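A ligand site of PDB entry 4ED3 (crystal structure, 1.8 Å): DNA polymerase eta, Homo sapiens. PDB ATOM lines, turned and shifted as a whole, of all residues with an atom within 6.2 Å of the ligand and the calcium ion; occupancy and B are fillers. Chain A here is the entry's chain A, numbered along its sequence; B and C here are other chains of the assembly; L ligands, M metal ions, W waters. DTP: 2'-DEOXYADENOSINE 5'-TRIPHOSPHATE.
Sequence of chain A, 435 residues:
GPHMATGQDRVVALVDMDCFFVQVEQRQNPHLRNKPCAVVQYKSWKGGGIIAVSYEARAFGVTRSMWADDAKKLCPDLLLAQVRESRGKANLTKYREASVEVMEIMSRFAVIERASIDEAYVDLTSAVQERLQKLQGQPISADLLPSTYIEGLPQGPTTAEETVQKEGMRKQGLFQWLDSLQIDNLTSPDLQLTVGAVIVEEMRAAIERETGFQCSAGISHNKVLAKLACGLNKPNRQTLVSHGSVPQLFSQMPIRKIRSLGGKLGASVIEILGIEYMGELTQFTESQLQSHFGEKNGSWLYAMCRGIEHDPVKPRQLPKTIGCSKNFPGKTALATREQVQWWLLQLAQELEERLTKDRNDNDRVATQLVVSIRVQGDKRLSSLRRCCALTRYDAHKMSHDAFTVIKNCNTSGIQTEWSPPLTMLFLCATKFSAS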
ATOM      1  N   ASP A  16      35.008 -39.139   4.848  1.00  0.00           N
ATOM      2  CA  ASP A  16      34.269 -37.896   5.012  1.00  0.00           C
ATOM      3  C   ASP A  16      35.125 -36.821   5.669  1.00  0.00           C
ATOM      4  O   ASP A  16      35.709 -37.049   6.722  1.00  0.00           O
ATOM      5  CB  ASP A  16      33.047 -38.177   5.881  1.00  0.00           C
ATOM      6  CG  ASP A  16      32.377 -36.919   6.333  1.00  0.00           C
ATOM      7  OD1 ASP A  16      32.601 -36.512   7.483  1.00  0.00           O
ATOM      8  OD2 ASP A  16      31.646 -36.315   5.537  1.00  0.00           O
ATOM      9  N   MET A  17      35.190 -35.626   5.074  1.00  0.00           N
ATOM     10  CA  MET A  17      36.063 -34.576   5.615  1.00  0.00           C
ATOM     11  C   MET A  17      35.508 -34.068   6.942  1.00  0.00           C
ATOM     12  O   MET A  17      34.311 -33.951   7.116  1.00  0.00           O
ATOM     13  CB  MET A  17      36.171 -33.397   4.632  1.00  0.00           C
ATOM     14  CG  MET A  17      36.555 -33.786   3.201  1.00  0.00           C
ATOM     15  SD  MET A  17      38.053 -34.785   3.122  1.00  0.00           S
ATOM     16  CE  MET A  17      39.298 -33.681   3.701  1.00  0.00           C
ATOM     17  N   ASP A  18      36.381 -33.789   7.892  1.00  0.00           N
ATOM     18  CA  ASP A  18      35.917 -33.194   9.143  1.00  0.00           C
ATOM     19  C   ASP A  18      35.522 -31.726   8.953  1.00  0.00           C
ATOM     20  O   ASP A  18      36.229 -30.975   8.264  1.00  0.00           O
ATOM     21  CB  ASP A  18      37.014 -33.294  10.204  1.00  0.00           C
ATOM     22  CG  ASP A  18      37.423 -34.759  10.491  1.00  0.00           C
ATOM     23  OD1 ASP A  18      36.582 -35.669  10.365  1.00  0.00           O
ATOM     24  OD2 ASP A  18      38.586 -34.962  10.874  1.00  0.00           O
ATOM     25  N   CYS A  19      34.415 -31.324   9.580  1.00  0.00           N
ATOM     26  CA  CYS A  19      33.886 -29.948   9.501  1.00  0.00           C
ATOM     27  C   CYS A  19      34.339 -29.228   8.222  1.00  0.00           C
ATOM     28  O   CYS A  19      35.054 -28.246   8.278  1.00  0.00           O
ATOM     29  CB  CYS A  19      34.235 -29.120  10.746  1.00  0.00           C
ATOM     30  SG  CYS A  19      35.974 -29.090  11.260  1.00  0.00           S
ATOM     31  N   PHE A  20      33.877 -29.721   7.083  1.00  0.00           N
ATOM     32  CA  PHE A  20      34.542 -29.421   5.817  1.00  0.00           C
ATOM     33  C   PHE A  20      34.669 -27.921   5.494  1.00  0.00           C
ATOM     34  O   PHE A  20      35.772 -27.450   5.256  1.00  0.00           O
ATOM     35  CB  PHE A  20      33.883 -30.160   4.658  1.00  0.00           C
ATOM     36  CG  PHE A  20      34.564 -29.948   3.345  1.00  0.00           C
ATOM     37  CD1 PHE A  20      35.931 -30.120   3.214  1.00  0.00           C
ATOM     38  CD2 PHE A  20      33.827 -29.583   2.231  1.00  0.00           C
ATOM     39  CE1 PHE A  20      36.565 -29.940   1.974  1.00  0.00           C
ATOM     40  CE2 PHE A  20      34.435 -29.397   1.003  1.00  0.00           C
ATOM     41  CZ  PHE A  20      35.802 -29.569   0.873  1.00  0.00           C
ATOM     42  N   PHE A  21      33.565 -27.183   5.489  1.00  0.00           N
ATOM     43  CA  PHE A  21      33.659 -25.782   5.068  1.00  0.00           C
ATOM     44  C   PHE A  21      34.568 -25.000   6.028  1.00  0.00           C
ATOM     45  O   PHE A  21      35.238 -24.048   5.616  1.00  0.00           O
ATOM     46  CB  PHE A  21      32.301 -25.071   4.981  1.00  0.00           C
ATOM     47  CG  PHE A  21      31.435 -25.510   3.832  1.00  0.00           C
ATOM     48  CD1 PHE A  21      31.727 -26.668   3.119  1.00  0.00           C
ATOM     49  CD2 PHE A  21      30.329 -24.745   3.459  1.00  0.00           C
ATOM     50  CE1 PHE A  21      30.921 -27.052   2.053  1.00  0.00           C
ATOM     51  CE2 PHE A  21      29.521 -25.140   2.385  1.00  0.00           C
ATOM     52  CZ  PHE A  21      29.814 -26.295   1.703  1.00  0.00           C
ATOM     53  N   VAL A  22      34.547 -25.364   7.299  1.00  0.00           N
ATOM     54  CA  VAL A  22      35.469 -24.745   8.264  1.00  0.00           C
ATOM     55  C   VAL A  22      36.940 -25.001   7.893  1.00  0.00           C
ATOM     56  O   VAL A  22      37.752 -24.074   7.901  1.00  0.00           O
ATOM     57  CB  VAL A  22      35.191 -25.225   9.677  1.00  0.00           C
ATOM     58  CG1 VAL A  22      36.352 -24.847  10.602  1.00  0.00           C
ATOM     59  CG2 VAL A  22      33.887 -24.628  10.195  1.00  0.00           C
ATOM     60  N   GLN A  41      26.187 -18.095   6.553  1.00  0.00           N
ATOM     61  CA  GLN A  41      25.738 -17.438   5.330  1.00  0.00           C
ATOM     62  C   GLN A  41      24.777 -16.290   5.608  1.00  0.00           C
ATOM     63  O   GLN A  41      23.900 -16.388   6.463  1.00  0.00           O
ATOM     64  CB  GLN A  41      25.193 -18.426   4.285  1.00  0.00           C
ATOM     65  CG  GLN A  41      23.990 -19.231   4.686  1.00  0.00           C
ATOM     66  CD  GLN A  41      23.819 -20.462   3.792  1.00  0.00           C
ATOM     67  OE1 GLN A  41      24.584 -20.675   2.846  1.00  0.00           O
ATOM     68  NE2 GLN A  41      22.832 -21.275   4.095  1.00  0.00           N
ATOM     69  N   ILE A  51      26.412 -22.888   8.928  1.00  0.00           N
ATOM     70  CA  ILE A  51      26.361 -24.124   8.127  1.00  0.00           C
ATOM     71  C   ILE A  51      27.479 -25.135   8.410  1.00  0.00           C
ATOM     72  O   ILE A  51      27.394 -26.282   7.958  1.00  0.00           O
ATOM     73  CB  ILE A  51      26.245 -23.834   6.622  1.00  0.00           C
ATOM     74  CG1 ILE A  51      27.434 -23.022   6.111  1.00  0.00           C
ATOM     75  CG2 ILE A  51      24.923 -23.102   6.315  1.00  0.00           C
ATOM     76  CD1 ILE A  51      27.481 -22.921   4.588  1.00  0.00           C
ATOM     77  N   ALA A  52      28.515 -24.736   9.152  1.00  0.00           N
ATOM     78  CA  ALA A  52      29.609 -25.648   9.520  1.00  0.00           C
ATOM     79  C   ALA A  52      30.274 -25.172  10.805  1.00  0.00           C
ATOM     80  O   ALA A  52      30.399 -23.974  11.008  1.00  0.00           O
ATOM     81  CB  ALA A  52      30.656 -25.768   8.369  1.00  0.00           C
ATOM     82  N   VAL A  53      30.715 -26.108  11.656  1.00  0.00           N
ATOM     83  CA  VAL A  53      31.213 -25.758  12.990  1.00  0.00           C
ATOM     84  C   VAL A  53      32.470 -26.550  13.341  1.00  0.00           C
ATOM     85  O   VAL A  53      32.485 -27.770  13.186  1.00  0.00           O
ATOM     86  CB  VAL A  53      30.123 -26.037  14.058  1.00  0.00           C
ATOM     87  CG1 VAL A  53      30.586 -25.552  15.432  1.00  0.00           C
ATOM     88  CG2 VAL A  53      28.806 -25.391  13.669  1.00  0.00           C
ATOM     89  N   TYR A  55      35.338 -28.411  15.619  1.00  0.00           N
ATOM     90  CA  TYR A  55      35.152 -29.242  16.799  1.00  0.00           C
ATOM     91  C   TYR A  55      35.375 -28.470  18.094  1.00  0.00           C
ATOM     92  O   TYR A  55      34.683 -28.729  19.078  1.00  0.00           O
ATOM     93  CB  TYR A  55      36.001 -30.522  16.701  1.00  0.00           C
ATOM     94  CG  TYR A  55      35.339 -31.494  15.763  1.00  0.00           C
ATOM     95  CD1 TYR A  55      35.430 -31.332  14.383  1.00  0.00           C
ATOM     96  CD2 TYR A  55      34.563 -32.536  16.250  1.00  0.00           C
ATOM     97  CE1 TYR A  55      34.791 -32.213  13.521  1.00  0.00           C
ATOM     98  CE2 TYR A  55      33.930 -33.420  15.402  1.00  0.00           C
ATOM     99  CZ  TYR A  55      34.038 -33.254  14.045  1.00  0.00           C
ATOM    100  OH  TYR A  55      33.385 -34.158  13.218  1.00  0.00           O
ATOM    101  N   ARG A  58      32.087 -26.885  18.700  1.00  0.00           N
ATOM    102  CA  ARG A  58      31.041 -27.837  19.101  1.00  0.00           C
ATOM    103  C   ARG A  58      31.037 -28.088  20.600  1.00  0.00           C
ATOM    104  O   ARG A  58      29.982 -28.307  21.193  1.00  0.00           O
ATOM    105  CB  ARG A  58      31.211 -29.169  18.376  1.00  0.00           C
ATOM    106  CG  ARG A  58      31.052 -29.005  16.885  1.00  0.00           C
ATOM    107  CD  ARG A  58      31.235 -30.308  16.165  1.00  0.00           C
ATOM    108  NE  ARG A  58      31.393 -30.040  14.739  1.00  0.00           N
ATOM    109  CZ  ARG A  58      31.250 -30.950  13.786  1.00  0.00           C
ATOM    110  NH1 ARG A  58      30.942 -32.205  14.098  1.00  0.00           N
ATOM    111  NH2 ARG A  58      31.428 -30.592  12.510  1.00  0.00           N
ATOM    112  N   ARG A  64      25.084 -26.557  13.616  1.00  0.00           N
ATOM    113  CA  ARG A  64      24.487 -26.156  12.354  1.00  0.00           C
ATOM    114  C   ARG A  64      23.031 -25.692  12.555  1.00  0.00           C
ATOM    115  O   ARG A  64      22.334 -26.160  13.457  1.00  0.00           O
ATOM    116  CB  ARG A  64      24.554 -27.336  11.363  1.00  0.00           C
ATOM    117  CG  ARG A  64      23.796 -27.147  10.068  1.00  0.00           C
ATOM    118  CD  ARG A  64      24.090 -28.313   9.114  1.00  0.00           C
ATOM    119  NE  ARG A  64      25.507 -28.361   8.791  1.00  0.00           N
ATOM    120  CZ  ARG A  64      26.281 -29.448   8.900  1.00  0.00           C
ATOM    121  NH1 ARG A  64      25.769 -30.598   9.296  1.00  0.00           N
ATOM    122  NH2 ARG A  64      27.573 -29.368   8.589  1.00  0.00           N
ATOM    123  N   SER A 116      28.476 -36.732  -1.518  1.00  0.00           N
ATOM    124  CA  SER A 116      28.122 -35.362  -1.142  1.00  0.00           C
ATOM    125  C   SER A 116      29.320 -34.482  -1.446  1.00  0.00           C
ATOM    126  O   SER A 116      30.335 -34.962  -1.924  1.00  0.00           O
ATOM    127  CB  SER A 116      27.800 -35.304   0.350  1.00  0.00           C
ATOM    128  OG  SER A 116      28.982 -35.412   1.114  1.00  0.00           O
ATOM    129  N   ILE A 117      29.220 -33.189  -1.150  1.00  0.00           N
ATOM    130  CA  ILE A 117      30.327 -32.281  -1.399  1.00  0.00           C
ATOM    131  C   ILE A 117      31.617 -32.714  -0.681  1.00  0.00           C
ATOM    132  O   ILE A 117      32.716 -32.385  -1.125  1.00  0.00           O
ATOM    133  CB  ILE A 117      29.977 -30.827  -1.001  1.00  0.00           C
ATOM    134  CG1 ILE A 117      31.008 -29.852  -1.582  1.00  0.00           C
ATOM    135  CG2 ILE A 117      29.884 -30.687   0.499  1.00  0.00           C
ATOM    136  CD1 ILE A 117      30.496 -28.418  -1.683  1.00  0.00           C
ATOM    137  N   ASP A 118      31.516 -33.453   0.418  1.00  0.00           N
ATOM    138  CA  ASP A 118      32.742 -33.746   1.168  1.00  0.00           C
ATOM    139  C   ASP A 118      32.931 -35.214   1.544  1.00  0.00           C
ATOM    140  O   ASP A 118      33.733 -35.554   2.433  1.00  0.00           O
ATOM    141  CB  ASP A 118      32.791 -32.882   2.420  1.00  0.00           C
ATOM    142  CG  ASP A 118      32.008 -33.468   3.556  1.00  0.00           C
ATOM    143  OD1 ASP A 118      32.483 -33.296   4.678  1.00  0.00           O
ATOM    144  OD2 ASP A 118      30.954 -34.111   3.342  1.00  0.00           O
ATOM    145  N   GLU A 119      32.204 -36.099   0.876  1.00  0.00           N
ATOM    146  CA  GLU A 119      32.390 -37.514   1.184  1.00  0.00           C
ATOM    147  C   GLU A 119      32.246 -38.409  -0.028  1.00  0.00           C
ATOM    148  O   GLU A 119      31.539 -38.079  -0.988  1.00  0.00           O
ATOM    149  CB  GLU A 119      31.449 -37.958   2.278  1.00  0.00           C
ATOM    150  CG  GLU A 119      30.055 -38.212   1.828  1.00  0.00           C
ATOM    151  CD  GLU A 119      29.094 -38.287   2.998  1.00  0.00           C
ATOM    152  OE1 GLU A 119      28.705 -37.225   3.503  1.00  0.00           O
ATOM    153  OE2 GLU A 119      28.744 -39.408   3.402  1.00  0.00           O
ATOM    154  N   LYS A 227      29.389 -46.012   6.393  1.00  0.00           N
ATOM    155  CA  LYS A 227      28.921 -44.685   6.808  1.00  0.00           C
ATOM    156  C   LYS A 227      28.718 -44.605   8.310  1.00  0.00           C
ATOM    157  O   LYS A 227      29.157 -43.649   8.947  1.00  0.00           O
ATOM    158  CB  LYS A 227      27.617 -44.303   6.080  1.00  0.00           C
ATOM    159  CG  LYS A 227      27.015 -42.939   6.487  1.00  0.00           C
ATOM    160  CD  LYS A 227      27.956 -41.774   6.206  1.00  0.00           C
ATOM    161  CE  LYS A 227      27.251 -40.438   6.427  1.00  0.00           C
ATOM    162  NZ  LYS A 227      28.180 -39.279   6.325  1.00  0.00           N
ATOM    163  N   LYS A 234      35.062 -39.522  15.367  1.00  0.00           N
ATOM    164  CA  LYS A 234      35.446 -38.318  14.652  1.00  0.00           C
ATOM    165  C   LYS A 234      35.918 -37.375  15.724  1.00  0.00           C
ATOM    166  O   LYS A 234      35.480 -37.489  16.874  1.00  0.00           O
ATOM    167  CB  LYS A 234      34.228 -37.690  13.951  1.00  0.00           C
ATOM    168  CG  LYS A 234      33.967 -38.156  12.522  1.00  0.00           C
ATOM    169  CD  LYS A 234      32.989 -37.204  11.820  1.00  0.00           C
ATOM    170  CE  LYS A 234      33.000 -37.355  10.294  1.00  0.00           C
ATOM    171  NZ  LYS A 234      33.910 -36.364   9.607  1.00  0.00           N
ATOM    172  N   PRO A 235      36.814 -36.427  15.385  1.00  0.00           N
ATOM    173  CA  PRO A 235      37.387 -36.219  14.059  1.00  0.00           C
ATOM    174  C   PRO A 235      38.738 -36.912  13.874  1.00  0.00           C
ATOM    175  O   PRO A 235      39.325 -37.413  14.854  1.00  0.00           O
ATOM    176  CB  PRO A 235      37.614 -34.710  14.031  1.00  0.00           C
ATOM    177  CG  PRO A 235      38.010 -34.390  15.456  1.00  0.00           C
ATOM    178  CD  PRO A 235      37.206 -35.355  16.319  1.00  0.00           C
ATOM    179  P    DT B   3      13.397 -20.284  11.037  1.00  0.00           P
ATOM    180  OP1  DT B   3      11.972 -20.319  11.412  1.00  0.00           O
ATOM    181  OP2  DT B   3      14.445 -20.414  12.084  1.00  0.00           O
ATOM    182  O5'  DT B   3      13.630 -21.406   9.929  1.00  0.00           O
ATOM    183  C5'  DT B   3      14.896 -22.037   9.804  1.00  0.00           C
ATOM    184  C4'  DT B   3      15.834 -21.202   8.965  1.00  0.00           C
ATOM    185  O4'  DT B   3      17.189 -21.683   9.158  1.00  0.00           O
ATOM    186  C3'  DT B   3      15.577 -21.250   7.466  1.00  0.00           C
ATOM    187  O3'  DT B   3      15.762 -19.972   6.908  1.00  0.00           O
ATOM    188  C2'  DT B   3      16.616 -22.240   6.941  1.00  0.00           C
ATOM    189  C1'  DT B   3      17.773 -22.010   7.905  1.00  0.00           C
ATOM    190  N1   DT B   3      18.627 -23.206   8.115  1.00  0.00           N
ATOM    191  C2   DT B   3      19.986 -23.151   7.847  1.00  0.00           C
ATOM    192  O2   DT B   3      20.547 -22.153   7.440  1.00  0.00           O
ATOM    193  N3   DT B   3      20.670 -24.319   8.095  1.00  0.00           N
ATOM    194  C4   DT B   3      20.130 -25.514   8.560  1.00  0.00           C
ATOM    195  O4   DT B   3      20.815 -26.510   8.752  1.00  0.00           O
ATOM    196  C5   DT B   3      18.704 -25.504   8.817  1.00  0.00           C
ATOM    197  C7   DT B   3      18.016 -26.730   9.331  1.00  0.00           C
ATOM    198  C6   DT B   3      18.031 -24.365   8.590  1.00  0.00           C
ATOM    199  P    DT B   4      15.620 -19.758   5.323  1.00  0.00           P
ATOM    200  OP1  DT B   4      15.481 -18.305   5.079  1.00  0.00           O
ATOM    201  OP2  DT B   4      14.618 -20.709   4.822  1.00  0.00           O
ATOM    202  O5'  DT B   4      17.043 -20.222   4.764  1.00  0.00           O
ATOM    203  C5'  DT B   4      18.176 -19.378   4.889  1.00  0.00           C
ATOM    204  C4'  DT B   4      19.218 -19.856   3.898  1.00  0.00           C
ATOM    205  O4'  DT B   4      19.741 -21.136   4.331  1.00  0.00           O
ATOM    206  C3'  DT B   4      18.708 -20.090   2.488  1.00  0.00           C
ATOM    207  O3'  DT B   4      19.732 -19.568   1.678  1.00  0.00           O
ATOM    208  C2'  DT B   4      18.544 -21.609   2.373  1.00  0.00           C
ATOM    209  C1'  DT B   4      19.690 -22.073   3.257  1.00  0.00           C
ATOM    210  N1   DT B   4      19.554 -23.380   3.929  1.00  0.00           N
ATOM    211  C2   DT B   4      20.705 -24.110   4.049  1.00  0.00           C
ATOM    212  O2   DT B   4      21.783 -23.755   3.604  1.00  0.00           O
ATOM    213  N3   DT B   4      20.544 -25.309   4.697  1.00  0.00           N
ATOM    214  C4   DT B   4      19.388 -25.816   5.239  1.00  0.00           C
ATOM    215  O4   DT B   4      19.371 -26.902   5.815  1.00  0.00           O
ATOM    216  C5   DT B   4      18.215 -24.992   5.100  1.00  0.00           C
ATOM    217  C7   DT B   4      16.913 -25.487   5.659  1.00  0.00           C
ATOM    218  C6   DT B   4      18.350 -23.810   4.461  1.00  0.00           C
ATOM    219  P    DA B   5      19.614 -19.610   0.082  1.00  0.00           P
ATOM    220  OP1  DA B   5      20.232 -18.388  -0.447  1.00  0.00           O
ATOM    221  OP2  DA B   5      18.239 -19.993  -0.265  1.00  0.00           O
ATOM    222  O5'  DA B   5      20.523 -20.857  -0.308  1.00  0.00           O
ATOM    223  C5'  DA B   5      21.945 -20.755  -0.161  1.00  0.00           C
ATOM    224  C4'  DA B   5      22.593 -22.011  -0.713  1.00  0.00           C
ATOM    225  O4'  DA B   5      22.282 -23.150   0.128  1.00  0.00           O
ATOM    226  C3'  DA B   5      22.119 -22.387  -2.119  1.00  0.00           C
ATOM    227  O3'  DA B   5      23.245 -22.817  -2.871  1.00  0.00           O
ATOM    228  C2'  DA B   5      21.148 -23.536  -1.860  1.00  0.00           C
ATOM    229  C1'  DA B   5      21.820 -24.208  -0.666  1.00  0.00           C
ATOM    230  N9   DA B   5      20.918 -25.022   0.144  1.00  0.00           N
ATOM    231  C8   DA B   5      19.623 -24.754   0.456  1.00  0.00           C
ATOM    232  N7   DA B   5      19.066 -25.674   1.225  1.00  0.00           N
ATOM    233  C5   DA B   5      20.084 -26.594   1.429  1.00  0.00           C
ATOM    234  C6   DA B   5      20.135 -27.801   2.149  1.00  0.00           C
ATOM    235  N6   DA B   5      19.096 -28.295   2.820  1.00  0.00           N
ATOM    236  N1   DA B   5      21.299 -28.482   2.152  1.00  0.00           N
ATOM    237  C2   DA B   5      22.335 -27.975   1.476  1.00  0.00           C
ATOM    238  N3   DA B   5      22.409 -26.848   0.753  1.00  0.00           N
ATOM    239  C4   DA B   5      21.236 -26.206   0.780  1.00  0.00           C
ATOM    240  P    DT C   8      23.556 -37.091   6.274  1.00  0.00           P
ATOM    241  OP1  DT C   8      24.617 -37.901   6.914  1.00  0.00           O
ATOM    242  OP2  DT C   8      22.691 -36.210   7.101  1.00  0.00           O
ATOM    243  O5'  DT C   8      24.227 -36.170   5.149  1.00  0.00           O
ATOM    244  C5'  DT C   8      25.048 -36.650   4.065  1.00  0.00           C
ATOM    245  C4'  DT C   8      25.607 -35.408   3.400  1.00  0.00           C
ATOM    246  O4'  DT C   8      24.437 -34.602   3.129  1.00  0.00           O
ATOM    247  C3'  DT C   8      26.415 -34.625   4.433  1.00  0.00           C
ATOM    248  O3'  DT C   8      27.656 -34.297   3.841  1.00  0.00           O
ATOM    249  C2'  DT C   8      25.577 -33.373   4.742  1.00  0.00           C
ATOM    250  C1'  DT C   8      24.685 -33.270   3.504  1.00  0.00           C
ATOM    251  N1   DT C   8      23.379 -32.612   3.740  1.00  0.00           N
ATOM    252  C2   DT C   8      23.103 -31.433   3.083  1.00  0.00           C
ATOM    253  O2   DT C   8      23.886 -30.919   2.316  1.00  0.00           O
ATOM    254  N3   DT C   8      21.876 -30.893   3.348  1.00  0.00           N
ATOM    255  C4   DT C   8      20.927 -31.410   4.194  1.00  0.00           C
ATOM    256  O4   DT C   8      19.849 -30.865   4.396  1.00  0.00           O
ATOM    257  C5   DT C   8      21.276 -32.645   4.862  1.00  0.00           C
ATOM    258  C7   DT C   8      20.318 -33.299   5.807  1.00  0.00           C
ATOM    259  C6   DT C   8      22.479 -33.182   4.602  1.00  0.00           C
HETATM  260  PG  DTP L   1      31.532 -33.413  10.316  1.00  0.00           P
HETATM  261  O1G DTP L   1      30.537 -33.714  11.423  1.00  0.00           O
HETATM  262  O2G DTP L   1      32.966 -33.350  10.784  1.00  0.00           O
HETATM  263  O3G DTP L   1      31.326 -34.312   9.134  1.00  0.00           O
HETATM  264  PB  DTP L   1      30.839 -31.351   8.414  1.00  0.00           P
HETATM  265  O1B DTP L   1      31.847 -31.901   7.434  1.00  0.00           O
HETATM  266  O2B DTP L   1      30.671 -29.849   8.510  1.00  0.00           O
HETATM  267  O3B DTP L   1      31.127 -31.895   9.909  1.00  0.00           O
HETATM  268  PA  DTP L   1      28.759 -32.744   6.896  1.00  0.00           P
HETATM  269  O1A DTP L   1      27.333 -33.122   7.290  1.00  0.00           O
HETATM  270  O2A DTP L   1      29.653 -33.837   6.430  1.00  0.00           O
HETATM  271  O3A DTP L   1      29.368 -31.990   8.210  1.00  0.00           O
HETATM  272  O5' DTP L   1      28.604 -31.671   5.734  1.00  0.00           O
HETATM  273  C5' DTP L   1      29.704 -31.294   4.917  1.00  0.00           C
HETATM  274  C4' DTP L   1      29.570 -29.827   4.522  1.00  0.00           C
HETATM  275  O4' DTP L   1      28.379 -29.604   3.767  1.00  0.00           O
HETATM  276  C3' DTP L   1      29.493 -28.891   5.704  1.00  0.00           C
HETATM  277  O3' DTP L   1      30.810 -28.476   6.093  1.00  0.00           O
HETATM  278  C2' DTP L   1      28.657 -27.734   5.169  1.00  0.00           C
HETATM  279  C1' DTP L   1      27.722 -28.386   4.158  1.00  0.00           C
HETATM  280  N9  DTP L   1      26.401 -28.722   4.754  1.00  0.00           N
HETATM  281  C8  DTP L   1      26.100 -29.823   5.471  1.00  0.00           C
HETATM  282  N7  DTP L   1      24.790 -29.754   5.834  1.00  0.00           N
HETATM  283  C5  DTP L   1      24.276 -28.607   5.333  1.00  0.00           C
HETATM  284  C6  DTP L   1      23.021 -27.994   5.370  1.00  0.00           C
HETATM  285  N6  DTP L   1      21.999 -28.597   6.022  1.00  0.00           N
HETATM  286  N1  DTP L   1      22.822 -26.800   4.758  1.00  0.00           N
HETATM  287  C2  DTP L   1      23.832 -26.212   4.118  1.00  0.00           C
HETATM  288  N3  DTP L   1      25.062 -26.776   4.062  1.00  0.00           N
HETATM  289  C4  DTP L   1      25.305 -27.964   4.661  1.00  0.00           C
HETATM  290 CA    CA M   1      32.000 -34.142   6.886  1.00  0.00          CA
HETATM  291  O   HOH W   1      29.671 -36.458   9.104  1.00  0.00           O
HETATM  292  O   HOH W   2      29.909 -28.643  10.832  1.00  0.00           O
HETATM  293  O   HOH W   3      26.254 -25.476   1.754  1.00  0.00           O
HETATM  294  O   HOH W   4      28.148 -32.701  11.836  1.00  0.00           O
HETATM  295  O   HOH W   5      20.964 -30.510   8.605  1.00  0.00           O
HETATM  296  O   HOH W   6      27.652 -32.169   2.438  1.00  0.00           O
HETATM  297  O   HOH W   7      29.580 -35.927  12.397  1.00  0.00           O
HETATM  298  O   HOH W   8      26.101 -29.555   1.443  1.00  0.00           O
HETATM  299  O   HOH W   9      27.951 -36.397   7.032  1.00  0.00           O
HETATM  300  O   HOH W  10      23.009 -31.193   7.462  1.00  0.00           O
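The calcium ion is bound by an oxygen (O1B) of the ligand (2.3 Å), the backbone carbonyl oxygen (O) of Met 17 (2.3 Å), an oxygen (O3G) of the ligand (2.4 Å), an oxygen (O2A) of the ligand (2.4 Å), the side-chain carboxylate (OD1) of Asp 118 (2.4 Å), the side-chain carboxylate (OD1) of Asp 16 (2.5 Å) and the side-chain carboxylate (OD2) of Asp 16 (2.6 Å).
The calcium ion has seven donor atoms within binding distance.
O of Met 17 sits close to NZ of Lys 234 (3.5 Å).
OD2 of Asp 118 sits at hydrogen-bond distance from OG of Ser 116 (3.2 Å).
The side-chain amino group of Lys 234 lies within hydrogen-bond range of the backbone carbonyl oxygen of Asp 16 (3.5 Å).
The side-chain hydroxyl (OH) of Tyr 55 lies within hydrogen-bond range of the guanidinium group (NH1) of Arg 58 (3.2 Å).
O2 of DT 4 of chain B sits at hydrogen-bond distance from the side-chain amide nitrogen (NE2) of Gln 41 (2.7 Å).
NE of Arg 58 is in hydrogen-bond range of O of Val 53 (3.0 Å).
O3' of DT 8 of chain C lies within hydrogen-bond range of OG of Ser 116 (3.2 Å).
NE of Arg 64 is in hydrogen-bond range of O of Ile 51, 2.9 Å away.
OH of Tyr 55 sits at hydrogen-bond distance from O2G of the ligand, 2.6 Å away.
O4 of DT 4 of chain B is in hydrogen-bond range of N6 of the ligand.
N of Cys 19 sits at hydrogen-bond distance from O2G of the ligand (2.8 Å).
An oxygen (O1G) of the ligand is in salt-bridge range of the guanidinium group of Arg 58 (3.1 Å).
An oxygen (O3') of the ligand lies within hydrogen-bond range of the backbone NH of Phe 20, at 3.5 Å.
The backbone NH (N) of Phe 21 sits at hydrogen-bond distance from an oxygen (O3') of the ligand (3.1 Å).
O2B of the ligand is in salt-bridge range of NH2 of Arg 64 (3.1 Å).
The side-chain amino group of Lys 234 is in salt-bridge range of an oxygen (O2G) of the ligand, 3.4 Å away.
Water W10 lies within hydrogen-bond range of a nitrogen (N7) of the ligand and the guanidinium group (NH1) of Arg 64.
Water W6 bridges O3' of DT 8 of chain C (2.5 Å) and an oxygen (O4') of the ligand (3.0 Å).
Water W9 bridges NZ of Lys 227 and O1A of the ligand.
Water W8 lies within hydrogen-bond range of O2 of DT 8 of chain C (2.7 Å) and an oxygen (O4') of the ligand (3.3 Å).
NZ of Lys 234 touches the calcium ion, at 3.999 Å.
Within 4 Å of the calcium ion: Asp 16, Met 17, Asp 118 and Lys 234.
The nearest printed residue that does not touch the calcium ion is Asp 18 (4.5 Å).
A nitrogen (N1) of the ligand lies close to N1 of DA 5 of chain B (3.5 Å).
O3' of DT 8 of chain C sits close to an oxygen (O2A) of the ligand (3.3 Å).
Merely in contact with the ligand: Asp 18, Ile 51, Ala 52, DT 3 of chain B and Ile 117.
Hydrophobic or aromatic side chains that line the ligand: Phe 20, Phe 21, Ile 51, Ala 52, Tyr 55 and Ile 117.
Of the 25 residues printed, 18 come within 4 Å of the ligand.
The nearest printed residue that does not touch the ligand is Glu 119 (4.6 Å).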
